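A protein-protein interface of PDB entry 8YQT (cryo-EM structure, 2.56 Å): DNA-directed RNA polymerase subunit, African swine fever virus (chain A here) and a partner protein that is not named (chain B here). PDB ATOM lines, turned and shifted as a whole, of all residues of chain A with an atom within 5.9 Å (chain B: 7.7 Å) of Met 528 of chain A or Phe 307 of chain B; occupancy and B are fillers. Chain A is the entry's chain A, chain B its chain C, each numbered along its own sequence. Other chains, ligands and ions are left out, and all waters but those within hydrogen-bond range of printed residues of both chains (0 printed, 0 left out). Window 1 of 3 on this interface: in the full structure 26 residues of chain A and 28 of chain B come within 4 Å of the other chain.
Of the 13 printed residues of chain A, 7 touch a printed residue of chain B. Printed residues of chain A that touch a printed residue of chain B: Lys 524, Leu 525, Met 528, Gln 532, Pro 538, Pro 539 and Phe 541. Hydrophobic or aromatic side chains of chain A that line the printed part of chain B: Leu 525, Met 528, Pro 538 and Phe 541. Among the printed residues, 19 pairs touch across the chains.
Printed residues of chain B within 4 Å of Met 528 of chain A: Tyr 299, Phe 307 and Val 308. Of chain A, only Met 528, Gln 532 and Pro 538 come within 4 Å of Phe 307 of chain B. Of the printed residues of chain B, Pro 539 of chain A touches Ser 306 (3.6 Å). Of the printed residues of chain A, Tyr 310 of chain B touches Gln 532 (3.6 Å). Printed residues of chain B within 4 Å of Gln 532 of chain A: Lys 295, Phe 307, Gly 309, Tyr 310 and Gln 311. Of the printed residues of chain A, Pro 303 of chain B touches Lys 524. Of the printed residues of chain A, Lys 295 of chain B touches Leu 525 and Gln 532. Lys 278 of chain B touches none of the printed residues of chain A. The nearest residue of chain B that does not touch Met 528 of chain A is Ser 306 of chain B (4.2 Å). The nearest residue of chain A that does not touch Phe 307 of chain B is Phe 531 of chain A (4.1 Å).
Tyr 299 of chain B touches Lys 524 of chain A. Asp 304 of chain B touches Lys 524 of chain A. Tyr 299 of chain B touches Leu 525 of chain A. Met 528 of chain A touches Tyr 299 of chain B. Phe 307 of chain B touches Met 528 of chain A. Gly 309 of chain B touches Gln 532 of chain A (CA to OE1, 3.5 Å). Gln 532 of chain A touches Tyr 310 of chain B. Gln 532 of chain A touches Gln 311 of chain B. Ser 306 of chain B touches Pro 539 of chain A (O to O, 3.6 Å). Phe 541 of chain A touches Ile 305 of chain B (O to O, 3.6 Å).
The side-chain amino group (NZ) of Lys 524 of chain A sits at hydrogen-bond distance from the backbone carbonyl oxygen (O) of Pro 303 of chain B (2.9 Å). The side-chain amino group (NZ) of Lys 524 of chain A is in hydrogen-bond range of the backbone carbonyl oxygen (O) of Ile 305 of chain B, at 2.9 Å. N of Phe 541 of chain A is in hydrogen-bond range of O of Ser 306 of chain B (3.0 Å).
The side-chain amino group (NZ) of Lys 524 of chain A sits at hydrogen-bond distance from the backbone carbonyl oxygen (O) of Phe 541 of chain A (3.1 Å). The side-chain amide nitrogen (NE2) of Gln 532 of chain A sits close to the backbone carbonyl oxygen (O) of Gly 529 of chain A, at 3.5 Å. N of Ser 306 of chain B lies within hydrogen-bond range of O of Ile 324 of chain B (3.1 Å). The backbone carbonyl oxygen of Phe 307 of chain B lies within hydrogen-bond range of the backbone NH of Ile 324 of chain B (2.9 Å). The backbone carbonyl oxygen (O) of Gly 309 of chain B lies within hydrogen-bond range of the backbone NH (N) of Thr 322 of chain B (2.9 Å).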
ATOM      1  N   ASN A 523      12.097  15.003 -19.709  1.00  0.00           N
ATOM      2  CA  ASN A 523      12.283  16.236 -18.957  1.00  0.00           C
ATOM      3  C   ASN A 523      10.918  16.827 -18.602  1.00  0.00           C
ATOM      4  O   ASN A 523       9.868  16.265 -18.919  1.00  0.00           O
ATOM      5  CB  ASN A 523      13.163  17.207 -19.739  1.00  0.00           C
ATOM      6  CG  ASN A 523      12.615  17.520 -21.109  1.00  0.00           C
ATOM      7  OD1 ASN A 523      11.554  17.039 -21.492  1.00  0.00           O
ATOM      8  ND2 ASN A 523      13.338  18.339 -21.858  1.00  0.00           N
ATOM      9  N   LYS A 524      10.924  17.979 -17.928  1.00  0.00           N
ATOM     10  CA  LYS A 524       9.675  18.590 -17.484  1.00  0.00           C
ATOM     11  C   LYS A 524       8.791  18.981 -18.660  1.00  0.00           C
ATOM     12  O   LYS A 524       7.572  18.787 -18.616  1.00  0.00           O
ATOM     13  CB  LYS A 524       9.970  19.808 -16.610  1.00  0.00           C
ATOM     14  CG  LYS A 524       8.746  20.627 -16.254  1.00  0.00           C
ATOM     15  CD  LYS A 524       9.123  21.827 -15.415  1.00  0.00           C
ATOM     16  CE  LYS A 524       7.915  22.674 -15.088  1.00  0.00           C
ATOM     17  NZ  LYS A 524       8.258  23.738 -14.116  1.00  0.00           N
ATOM     18  N   LEU A 525       9.387  19.530 -19.719  1.00  0.00           N
ATOM     19  CA  LEU A 525       8.606  19.981 -20.865  1.00  0.00           C
ATOM     20  C   LEU A 525       7.871  18.830 -21.536  1.00  0.00           C
ATOM     21  O   LEU A 525       6.718  18.981 -21.950  1.00  0.00           O
ATOM     22  CB  LEU A 525       9.515  20.684 -21.868  1.00  0.00           C
ATOM     23  CG  LEU A 525       8.830  21.307 -23.081  1.00  0.00           C
ATOM     24  CD1 LEU A 525       7.907  22.437 -22.664  1.00  0.00           C
ATOM     25  CD2 LEU A 525       9.868  21.795 -24.067  1.00  0.00           C
ATOM     26  N   HIS A 526       8.521  17.677 -21.667  1.00  0.00           N
ATOM     27  CA  HIS A 526       7.891  16.554 -22.343  1.00  0.00           C
ATOM     28  C   HIS A 526       6.955  15.774 -21.434  1.00  0.00           C
ATOM     29  O   HIS A 526       6.054  15.096 -21.935  1.00  0.00           O
ATOM     30  CB  HIS A 526       8.960  15.631 -22.923  1.00  0.00           C
ATOM     31  CG  HIS A 526       9.638  16.199 -24.128  1.00  0.00           C
ATOM     32  ND1 HIS A 526      10.765  16.985 -24.046  1.00  0.00           N
ATOM     33  CD2 HIS A 526       9.323  16.128 -25.441  1.00  0.00           C
ATOM     34  CE1 HIS A 526      11.129  17.356 -25.260  1.00  0.00           C
ATOM     35  NE2 HIS A 526      10.271  16.849 -26.124  1.00  0.00           N
ATOM     36  N   ALA A 527       7.148  15.852 -20.117  1.00  0.00           N
ATOM     37  CA  ALA A 527       6.169  15.286 -19.199  1.00  0.00           C
ATOM     38  C   ALA A 527       4.895  16.120 -19.183  1.00  0.00           C
ATOM     39  O   ALA A 527       3.790  15.573 -19.110  1.00  0.00           O
ATOM     40  CB  ALA A 527       6.764  15.176 -17.798  1.00  0.00           C
ATOM     41  N   MET A 528       5.032  17.447 -19.246  1.00  0.00           N
ATOM     42  CA  MET A 528       3.861  18.310 -19.339  1.00  0.00           C
ATOM     43  C   MET A 528       3.113  18.101 -20.647  1.00  0.00           C
ATOM     44  O   MET A 528       1.895  18.296 -20.699  1.00  0.00           O
ATOM     45  CB  MET A 528       4.271  19.776 -19.207  1.00  0.00           C
ATOM     46  CG  MET A 528       4.178  20.331 -17.807  1.00  0.00           C
ATOM     47  SD  MET A 528       4.691  22.051 -17.675  1.00  0.00           S
ATOM     48  CE  MET A 528       5.902  22.158 -18.983  1.00  0.00           C
ATOM     49  N   GLY A 529       3.818  17.717 -21.708  1.00  0.00           N
ATOM     50  CA  GLY A 529       3.196  17.535 -23.004  1.00  0.00           C
ATOM     51  C   GLY A 529       2.362  16.285 -23.131  1.00  0.00           C
ATOM     52  O   GLY A 529       1.586  16.175 -24.084  1.00  0.00           O
ATOM     53  N   LEU A 530       2.508  15.336 -22.208  1.00  0.00           N
ATOM     54  CA  LEU A 530       1.668  14.148 -22.230  1.00  0.00           C
ATOM     55  C   LEU A 530       0.262  14.440 -21.730  1.00  0.00           C
ATOM     56  O   LEU A 530      -0.687  13.757 -22.127  1.00  0.00           O
ATOM     57  CB  LEU A 530       2.300  13.035 -21.394  1.00  0.00           C
ATOM     58  CG  LEU A 530       3.693  12.563 -21.805  1.00  0.00           C
ATOM     59  CD1 LEU A 530       4.082  11.341 -21.022  1.00  0.00           C
ATOM     60  CD2 LEU A 530       3.746  12.273 -23.284  1.00  0.00           C
ATOM     61  N   PHE A 531       0.110  15.443 -20.871  1.00  0.00           N
ATOM     62  CA  PHE A 531      -1.173  15.797 -20.284  1.00  0.00           C
ATOM     63  C   PHE A 531      -1.899  16.897 -21.039  1.00  0.00           C
ATOM     64  O   PHE A 531      -3.026  17.235 -20.670  1.00  0.00           O
ATOM     65  CB  PHE A 531      -0.978  16.229 -18.832  1.00  0.00           C
ATOM     66  CG  PHE A 531      -0.574  15.116 -17.923  1.00  0.00           C
ATOM     67  CD1 PHE A 531      -1.528  14.313 -17.329  1.00  0.00           C
ATOM     68  CD2 PHE A 531       0.759  14.867 -17.666  1.00  0.00           C
ATOM     69  CE1 PHE A 531      -1.159  13.290 -16.495  1.00  0.00           C
ATOM     70  CE2 PHE A 531       1.132  13.844 -16.833  1.00  0.00           C
ATOM     71  CZ  PHE A 531       0.172  13.055 -16.247  1.00  0.00           C
ATOM     72  N   GLN A 532      -1.303  17.457 -22.084  1.00  0.00           N
ATOM     73  CA  GLN A 532      -1.905  18.595 -22.763  1.00  0.00           C
ATOM     74  C   GLN A 532      -3.025  18.190 -23.711  1.00  0.00           C
ATOM     75  O   GLN A 532      -3.547  19.045 -24.430  1.00  0.00           O
ATOM     76  CB  GLN A 532      -0.835  19.390 -23.513  1.00  0.00           C
ATOM     77  CG  GLN A 532      -0.232  18.687 -24.702  1.00  0.00           C
ATOM     78  CD  GLN A 532       0.981  19.416 -25.236  1.00  0.00           C
ATOM     79  OE1 GLN A 532       1.353  20.471 -24.733  1.00  0.00           O
ATOM     80  NE2 GLN A 532       1.606  18.854 -26.260  1.00  0.00           N
ATOM     81  N   PRO A 538      -4.859  19.629 -15.478  1.00  0.00           N
ATOM     82  CA  PRO A 538      -3.426  19.369 -15.569  1.00  0.00           C
ATOM     83  C   PRO A 538      -2.814  19.193 -14.193  1.00  0.00           C
ATOM     84  O   PRO A 538      -3.213  19.869 -13.229  1.00  0.00           O
ATOM     85  CB  PRO A 538      -2.882  20.630 -16.266  1.00  0.00           C
ATOM     86  CG  PRO A 538      -4.056  21.225 -16.948  1.00  0.00           C
ATOM     87  CD  PRO A 538      -5.224  20.924 -16.073  1.00  0.00           C
ATOM     88  N   PRO A 539      -1.851  18.290 -14.047  1.00  0.00           N
ATOM     89  CA  PRO A 539      -1.150  18.157 -12.768  1.00  0.00           C
ATOM     90  C   PRO A 539      -0.251  19.356 -12.518  1.00  0.00           C
ATOM     91  O   PRO A 539      -0.045  20.212 -13.378  1.00  0.00           O
ATOM     92  CB  PRO A 539      -0.337  16.869 -12.934  1.00  0.00           C
ATOM     93  CG  PRO A 539      -0.979  16.152 -14.075  1.00  0.00           C
ATOM     94  CD  PRO A 539      -1.474  17.225 -14.986  1.00  0.00           C
ATOM     95  N   PHE A 541       3.328  20.802 -11.986  1.00  0.00           N
ATOM     96  CA  PHE A 541       4.736  20.561 -12.260  1.00  0.00           C
ATOM     97  C   PHE A 541       5.621  21.655 -11.676  1.00  0.00           C
ATOM     98  O   PHE A 541       6.761  21.826 -12.114  1.00  0.00           O
ATOM     99  CB  PHE A 541       4.967  20.440 -13.767  1.00  0.00           C
ATOM    100  CG  PHE A 541       4.406  19.184 -14.371  1.00  0.00           C
ATOM    101  CD1 PHE A 541       5.201  18.065 -14.537  1.00  0.00           C
ATOM    102  CD2 PHE A 541       3.087  19.123 -14.774  1.00  0.00           C
ATOM    103  CE1 PHE A 541       4.692  16.912 -15.095  1.00  0.00           C
ATOM    104  CE2 PHE A 541       2.571  17.974 -15.331  1.00  0.00           C
ATOM    105  CZ  PHE A 541       3.374  16.866 -15.489  1.00  0.00           C
ATOM    106  N   LYS B 276      -2.909  30.687  -7.141  1.00  0.00           N
ATOM    107  CA  LYS B 276      -2.713  30.044  -8.431  1.00  0.00           C
ATOM    108  C   LYS B 276      -3.670  30.641  -9.453  1.00  0.00           C
ATOM    109  O   LYS B 276      -4.866  30.785  -9.181  1.00  0.00           O
ATOM    110  CB  LYS B 276      -2.924  28.534  -8.322  1.00  0.00           C
ATOM    111  CG  LYS B 276      -2.279  27.731  -9.432  1.00  0.00           C
ATOM    112  CD  LYS B 276      -2.702  26.276  -9.364  1.00  0.00           C
ATOM    113  CE  LYS B 276      -1.979  25.522  -8.266  1.00  0.00           C
ATOM    114  NZ  LYS B 276      -0.576  25.215  -8.639  1.00  0.00           N
ATOM    115  N   THR B 277      -3.141  30.981 -10.623  1.00  0.00           N
ATOM    116  CA  THR B 277      -3.896  31.610 -11.696  1.00  0.00           C
ATOM    117  C   THR B 277      -3.838  30.732 -12.938  1.00  0.00           C
ATOM    118  O   THR B 277      -2.785  30.165 -13.262  1.00  0.00           O
ATOM    119  CB  THR B 277      -3.348  33.007 -12.007  1.00  0.00           C
ATOM    120  OG1 THR B 277      -3.391  33.809 -10.823  1.00  0.00           O
ATOM    121  CG2 THR B 277      -4.170  33.680 -13.091  1.00  0.00           C
ATOM    122  N   LYS B 278      -4.968  30.630 -13.629  1.00  0.00           N
ATOM    123  CA  LYS B 278      -5.095  29.856 -14.852  1.00  0.00           C
ATOM    124  C   LYS B 278      -5.530  30.764 -15.993  1.00  0.00           C
ATOM    125  O   LYS B 278      -6.419  31.598 -15.826  1.00  0.00           O
ATOM    126  CB  LYS B 278      -6.104  28.724 -14.667  1.00  0.00           C
ATOM    127  CG  LYS B 278      -6.247  27.804 -15.850  1.00  0.00           C
ATOM    128  CD  LYS B 278      -7.150  26.645 -15.501  1.00  0.00           C
ATOM    129  CE  LYS B 278      -7.209  25.634 -16.621  1.00  0.00           C
ATOM    130  NZ  LYS B 278      -8.010  24.447 -16.230  1.00  0.00           N
ATOM    131  N   ALA B 279      -4.892  30.609 -17.145  1.00  0.00           N
ATOM    132  CA  ALA B 279      -5.244  31.337 -18.352  1.00  0.00           C
ATOM    133  C   ALA B 279      -5.492  30.346 -19.478  1.00  0.00           C
ATOM    134  O   ALA B 279      -4.716  29.410 -19.678  1.00  0.00           O
ATOM    135  CB  ALA B 279      -4.142  32.319 -18.753  1.00  0.00           C
ATOM    136  N   LYS B 295       4.108  28.121 -26.381  1.00  0.00           N
ATOM    137  CA  LYS B 295       4.455  27.226 -25.284  1.00  0.00           C
ATOM    138  C   LYS B 295       5.946  27.275 -24.988  1.00  0.00           C
ATOM    139  O   LYS B 295       6.350  27.385 -23.824  1.00  0.00           O
ATOM    140  CB  LYS B 295       4.018  25.798 -25.604  1.00  0.00           C
ATOM    141  CG  LYS B 295       4.351  24.800 -24.513  1.00  0.00           C
ATOM    142  CD  LYS B 295       3.759  23.438 -24.795  1.00  0.00           C
ATOM    143  CE  LYS B 295       4.514  22.719 -25.891  1.00  0.00           C
ATOM    144  NZ  LYS B 295       5.869  22.304 -25.457  1.00  0.00           N
ATOM    145  N   ILE B 298       6.906  30.812 -23.411  1.00  0.00           N
ATOM    146  CA  ILE B 298       6.365  30.933 -22.063  1.00  0.00           C
ATOM    147  C   ILE B 298       7.136  30.034 -21.108  1.00  0.00           C
ATOM    148  O   ILE B 298       7.420  30.412 -19.966  1.00  0.00           O
ATOM    149  CB  ILE B 298       4.858  30.611 -22.058  1.00  0.00           C
ATOM    150  CG1 ILE B 298       4.071  31.725 -22.749  1.00  0.00           C
ATOM    151  CG2 ILE B 298       4.350  30.414 -20.643  1.00  0.00           C
ATOM    152  CD1 ILE B 298       2.684  31.313 -23.173  1.00  0.00           C
ATOM    153  N   TYR B 299       7.501  28.835 -21.567  1.00  0.00           N
ATOM    154  CA  TYR B 299       8.301  27.933 -20.750  1.00  0.00           C
ATOM    155  C   TYR B 299       9.700  28.486 -20.502  1.00  0.00           C
ATOM    156  O   TYR B 299      10.239  28.327 -19.403  1.00  0.00           O
ATOM    157  CB  TYR B 299       8.364  26.569 -21.428  1.00  0.00           C
ATOM    158  CG  TYR B 299       9.039  25.495 -20.624  1.00  0.00           C
ATOM    159  CD1 TYR B 299       8.556  25.133 -19.378  1.00  0.00           C
ATOM    160  CD2 TYR B 299      10.141  24.822 -21.121  1.00  0.00           C
ATOM    161  CE1 TYR B 299       9.162  24.145 -18.646  1.00  0.00           C
ATOM    162  CE2 TYR B 299      10.752  23.833 -20.395  1.00  0.00           C
ATOM    163  CZ  TYR B 299      10.259  23.499 -19.160  1.00  0.00           C
ATOM    164  OH  TYR B 299      10.866  22.509 -18.435  1.00  0.00           O
ATOM    165  N   ILE B 302       9.092  31.334 -17.881  1.00  0.00           N
ATOM    166  CA  ILE B 302       8.704  30.813 -16.574  1.00  0.00           C
ATOM    167  C   ILE B 302       9.184  29.372 -16.459  1.00  0.00           C
ATOM    168  O   ILE B 302       8.404  28.438 -16.691  1.00  0.00           O
ATOM    169  CB  ILE B 302       7.185  30.909 -16.362  1.00  0.00           C
ATOM    170  CG1 ILE B 302       6.666  32.266 -16.835  1.00  0.00           C
ATOM    171  CG2 ILE B 302       6.847  30.698 -14.902  1.00  0.00           C
ATOM    172  CD1 ILE B 302       5.171  32.319 -17.015  1.00  0.00           C
ATOM    173  N   PRO B 303      10.452  29.144 -16.109  1.00  0.00           N
ATOM    174  CA  PRO B 303      10.954  27.763 -16.023  1.00  0.00           C
ATOM    175  C   PRO B 303      10.255  26.913 -14.975  1.00  0.00           C
ATOM    176  O   PRO B 303      10.155  25.696 -15.166  1.00  0.00           O
ATOM    177  CB  PRO B 303      12.439  27.952 -15.693  1.00  0.00           C
ATOM    178  CG  PRO B 303      12.520  29.287 -15.060  1.00  0.00           C
ATOM    179  CD  PRO B 303      11.471  30.128 -15.715  1.00  0.00           C
ATOM    180  N   ASP B 304       9.772  27.501 -13.883  1.00  0.00           N
ATOM    181  CA  ASP B 304       9.106  26.758 -12.814  1.00  0.00           C
ATOM    182  C   ASP B 304       7.592  26.902 -12.881  1.00  0.00           C
ATOM    183  O   ASP B 304       6.917  26.976 -11.854  1.00  0.00           O
ATOM    184  CB  ASP B 304       9.627  27.204 -11.453  1.00  0.00           C
ATOM    185  CG  ASP B 304       9.454  28.692 -11.221  1.00  0.00           C
ATOM    186  OD1 ASP B 304       9.136  29.417 -12.187  1.00  0.00           O
ATOM    187  OD2 ASP B 304       9.628  29.138 -10.070  1.00  0.00           O
ATOM    188  N   ILE B 305       7.040  26.951 -14.093  1.00  0.00           N
ATOM    189  CA  ILE B 305       5.600  27.071 -14.261  1.00  0.00           C
ATOM    190  C   ILE B 305       4.910  25.783 -13.820  1.00  0.00           C
ATOM    191  O   ILE B 305       5.494  24.693 -13.822  1.00  0.00           O
ATOM    192  CB  ILE B 305       5.269  27.418 -15.721  1.00  0.00           C
ATOM    193  CG1 ILE B 305       3.898  28.086 -15.826  1.00  0.00           C
ATOM    194  CG2 ILE B 305       5.347  26.183 -16.605  1.00  0.00           C
ATOM    195  CD1 ILE B 305       3.675  28.768 -17.143  1.00  0.00           C
ATOM    196  N   SER B 306       3.650  25.918 -13.405  1.00  0.00           N
ATOM    197  CA  SER B 306       2.880  24.743 -13.011  1.00  0.00           C
ATOM    198  C   SER B 306       2.426  23.935 -14.218  1.00  0.00           C
ATOM    199  O   SER B 306       2.467  22.703 -14.185  1.00  0.00           O
ATOM    200  CB  SER B 306       1.677  25.153 -12.163  1.00  0.00           C
ATOM    201  OG  SER B 306       2.090  25.754 -10.951  1.00  0.00           O
ATOM    202  N   PHE B 307       1.986  24.599 -15.286  1.00  0.00           N
ATOM    203  CA  PHE B 307       1.619  23.875 -16.497  1.00  0.00           C
ATOM    204  C   PHE B 307       1.547  24.833 -17.675  1.00  0.00           C
ATOM    205  O   PHE B 307       1.196  26.001 -17.517  1.00  0.00           O
ATOM    206  CB  PHE B 307       0.279  23.151 -16.343  1.00  0.00           C
ATOM    207  CG  PHE B 307      -0.055  22.254 -17.496  1.00  0.00           C
ATOM    208  CD1 PHE B 307       0.500  20.995 -17.590  1.00  0.00           C
ATOM    209  CD2 PHE B 307      -0.915  22.676 -18.491  1.00  0.00           C
ATOM    210  CE1 PHE B 307       0.199  20.172 -18.651  1.00  0.00           C
ATOM    211  CE2 PHE B 307      -1.218  21.859 -19.554  1.00  0.00           C
ATOM    212  CZ  PHE B 307      -0.661  20.607 -19.634  1.00  0.00           C
ATOM    213  N   VAL B 308       1.861  24.311 -18.860  1.00  0.00           N
ATOM    214  CA  VAL B 308       1.618  25.015 -20.117  1.00  0.00           C
ATOM    215  C   VAL B 308       1.419  23.976 -21.218  1.00  0.00           C
ATOM    216  O   VAL B 308       2.153  22.989 -21.300  1.00  0.00           O
ATOM    217  CB  VAL B 308       2.759  26.008 -20.437  1.00  0.00           C
ATOM    218  CG1 VAL B 308       4.093  25.297 -20.573  1.00  0.00           C
ATOM    219  CG2 VAL B 308       2.438  26.813 -21.679  1.00  0.00           C
ATOM    220  N   GLY B 309       0.400  24.193 -22.048  1.00  0.00           N
ATOM    221  CA  GLY B 309       0.087  23.269 -23.126  1.00  0.00           C
ATOM    222  C   GLY B 309      -0.676  23.963 -24.227  1.00  0.00           C
ATOM    223  O   GLY B 309      -1.306  24.997 -23.999  1.00  0.00           O
ATOM    224  N   TYR B 310      -0.635  23.387 -25.436  1.00  0.00           N
ATOM    225  CA  TYR B 310      -1.108  24.086 -26.631  1.00  0.00           C
ATOM    226  C   TYR B 310      -1.993  23.214 -27.523  1.00  0.00           C
ATOM    227  O   TYR B 310      -1.822  23.192 -28.739  1.00  0.00           O
ATOM    228  CB  TYR B 310       0.070  24.656 -27.429  1.00  0.00           C
ATOM    229  CG  TYR B 310       0.821  23.671 -28.309  1.00  0.00           C
ATOM    230  CD1 TYR B 310       1.614  22.685 -27.758  1.00  0.00           C
ATOM    231  CD2 TYR B 310       0.735  23.739 -29.694  1.00  0.00           C
ATOM    232  CE1 TYR B 310       2.293  21.792 -28.558  1.00  0.00           C
ATOM    233  CE2 TYR B 310       1.402  22.850 -30.498  1.00  0.00           C
ATOM    234  CZ  TYR B 310       2.183  21.881 -29.927  1.00  0.00           C
ATOM    235  OH  TYR B 310       2.858  20.993 -30.733  1.00  0.00           O
ATOM    236  N   GLN B 311      -2.993  22.551 -26.960  1.00  0.00           N
ATOM    237  CA  GLN B 311      -3.741  21.560 -27.731  1.00  0.00           C
ATOM    238  C   GLN B 311      -4.384  22.162 -28.980  1.00  0.00           C
ATOM    239  O   GLN B 311      -5.200  23.079 -28.891  1.00  0.00           O
ATOM    240  CB  GLN B 311      -4.809  20.926 -26.843  1.00  0.00           C
ATOM    241  CG  GLN B 311      -5.487  19.723 -27.454  1.00  0.00           C
ATOM    242  CD  GLN B 311      -6.550  19.140 -26.551  1.00  0.00           C
ATOM    243  OE1 GLN B 311      -6.898  19.725 -25.527  1.00  0.00           O
ATOM    244  NE2 GLN B 311      -7.070  17.980 -26.923  1.00  0.00           N
ATOM    245  N   LEU B 321      -4.427  27.204 -25.673  1.00  0.00           N
ATOM    246  CA  LEU B 321      -3.237  27.282 -24.839  1.00  0.00           C
ATOM    247  C   LEU B 321      -3.664  27.440 -23.386  1.00  0.00           C
ATOM    248  O   LEU B 321      -4.355  28.401 -23.039  1.00  0.00           O
ATOM    249  CB  LEU B 321      -2.354  28.452 -25.271  1.00  0.00           C
ATOM    250  CG  LEU B 321      -1.000  28.640 -24.584  1.00  0.00           C
ATOM    251  CD1 LEU B 321       0.006  27.622 -25.072  1.00  0.00           C
ATOM    252  CD2 LEU B 321      -0.486  30.045 -24.813  1.00  0.00           C
ATOM    253  N   THR B 322      -3.250  26.499 -22.549  1.00  0.00           N
ATOM    254  CA  THR B 322      -3.546  26.499 -21.124  1.00  0.00           C
ATOM    255  C   THR B 322      -2.269  26.792 -20.350  1.00  0.00           C
ATOM    256  O   THR B 322      -1.243  26.140 -20.572  1.00  0.00           O
ATOM    257  CB  THR B 322      -4.129  25.156 -20.684  1.00  0.00           C
ATOM    258  OG1 THR B 322      -5.286  24.854 -21.471  1.00  0.00           O
ATOM    259  CG2 THR B 322      -4.520  25.196 -19.221  1.00  0.00           C
ATOM    260  N   ILE B 323      -2.340  27.770 -19.450  1.00  0.00           N
ATOM    261  CA  ILE B 323      -1.217  28.194 -18.624  1.00  0.00           C
ATOM    262  C   ILE B 323      -1.682  28.200 -17.177  1.00  0.00           C
ATOM    263  O   ILE B 323      -2.676  28.850 -16.848  1.00  0.00           O
ATOM    264  CB  ILE B 323      -0.705  29.587 -19.022  1.00  0.00           C
ATOM    265  CG1 ILE B 323      -0.345  29.626 -20.504  1.00  0.00           C
ATOM    266  CG2 ILE B 323       0.482  29.980 -18.173  1.00  0.00           C
ATOM    267  CD1 ILE B 323      -0.347  31.016 -21.082  1.00  0.00           C
ATOM    268  N   ILE B 324      -0.973  27.485 -16.313  1.00  0.00           N
ATOM    269  CA  ILE B 324      -1.257  27.476 -14.883  1.00  0.00           C
ATOM    270  C   ILE B 324       0.017  27.888 -14.166  1.00  0.00           C
ATOM    271  O   ILE B 324       1.065  27.255 -14.348  1.00  0.00           O
ATOM    272  CB  ILE B 324      -1.744  26.103 -14.402  1.00  0.00           C
ATOM    273  CG1 ILE B 324      -3.015  25.703 -15.149  1.00  0.00           C
ATOM    274  CG2 ILE B 324      -1.996  26.127 -12.916  1.00  0.00           C
ATOM    275  CD1 ILE B 324      -3.449  24.284 -14.897  1.00  0.00           C
ATOM    276  N   HIS B 325      -0.068  28.943 -13.358  1.00  0.00           N
ATOM    277  CA  HIS B 325       1.122  29.490 -12.722  1.00  0.00           C
ATOM    278  C   HIS B 325       0.756  30.052 -11.356  1.00  0.00           C
ATOM    279  O   HIS B 325      -0.395  30.403 -11.108  1.00  0.00           O
ATOM    280  CB  HIS B 325       1.769  30.562 -13.605  1.00  0.00           C
ATOM    281  CG  HIS B 325       3.004  31.168 -13.019  1.00  0.00           C
ATOM    282  ND1 HIS B 325       4.036  30.410 -12.510  1.00  0.00           N
ATOM    283  CD2 HIS B 325       3.384  32.460 -12.883  1.00  0.00           C
ATOM    284  CE1 HIS B 325       4.990  31.209 -12.070  1.00  0.00           C
ATOM    285  NE2 HIS B 325       4.620  32.458 -12.287  1.00  0.00           N
ATOM    286  N   LYS B 326       1.753  30.147 -10.476  1.00  0.00           N
ATOM    287  CA  LYS B 326       1.546  30.534  -9.084  1.00  0.00           C
ATOM    288  C   LYS B 326       1.647  32.037  -8.859  1.00  0.00           C
ATOM    289  O   LYS B 326       2.003  32.468  -7.755  1.00  0.00           O
ATOM    290  CB  LYS B 326       2.542  29.808  -8.180  1.00  0.00           C
ATOM    291  CG  LYS B 326       2.196  28.364  -7.887  1.00  0.00           C
ATOM    292  CD  LYS B 326       3.228  27.755  -6.955  1.00  0.00           C
ATOM    293  CE  LYS B 326       2.760  26.431  -6.389  1.00  0.00           C
ATOM    294  NZ  LYS B 326       1.984  25.658  -7.388  1.00  0.00           N
ATOM    295  N   LEU B 332       0.970  37.310 -14.275  1.00  0.00           N
ATOM    296  CA  LEU B 332       0.915  36.343 -15.363  1.00  0.00           C
ATOM    297  C   LEU B 332       0.830  37.038 -16.715  1.00  0.00           C
ATOM    298  O   LEU B 332       1.520  36.645 -17.663  1.00  0.00           O
ATOM    299  CB  LEU B 332      -0.267  35.396 -15.168  1.00  0.00           C
ATOM    300  CG  LEU B 332      -0.284  34.179 -16.094  1.00  0.00           C
ATOM    301  CD1 LEU B 332       0.941  33.317 -15.848  1.00  0.00           C
ATOM    302  CD2 LEU B 332      -1.555  33.366 -15.916  1.00  0.00           C
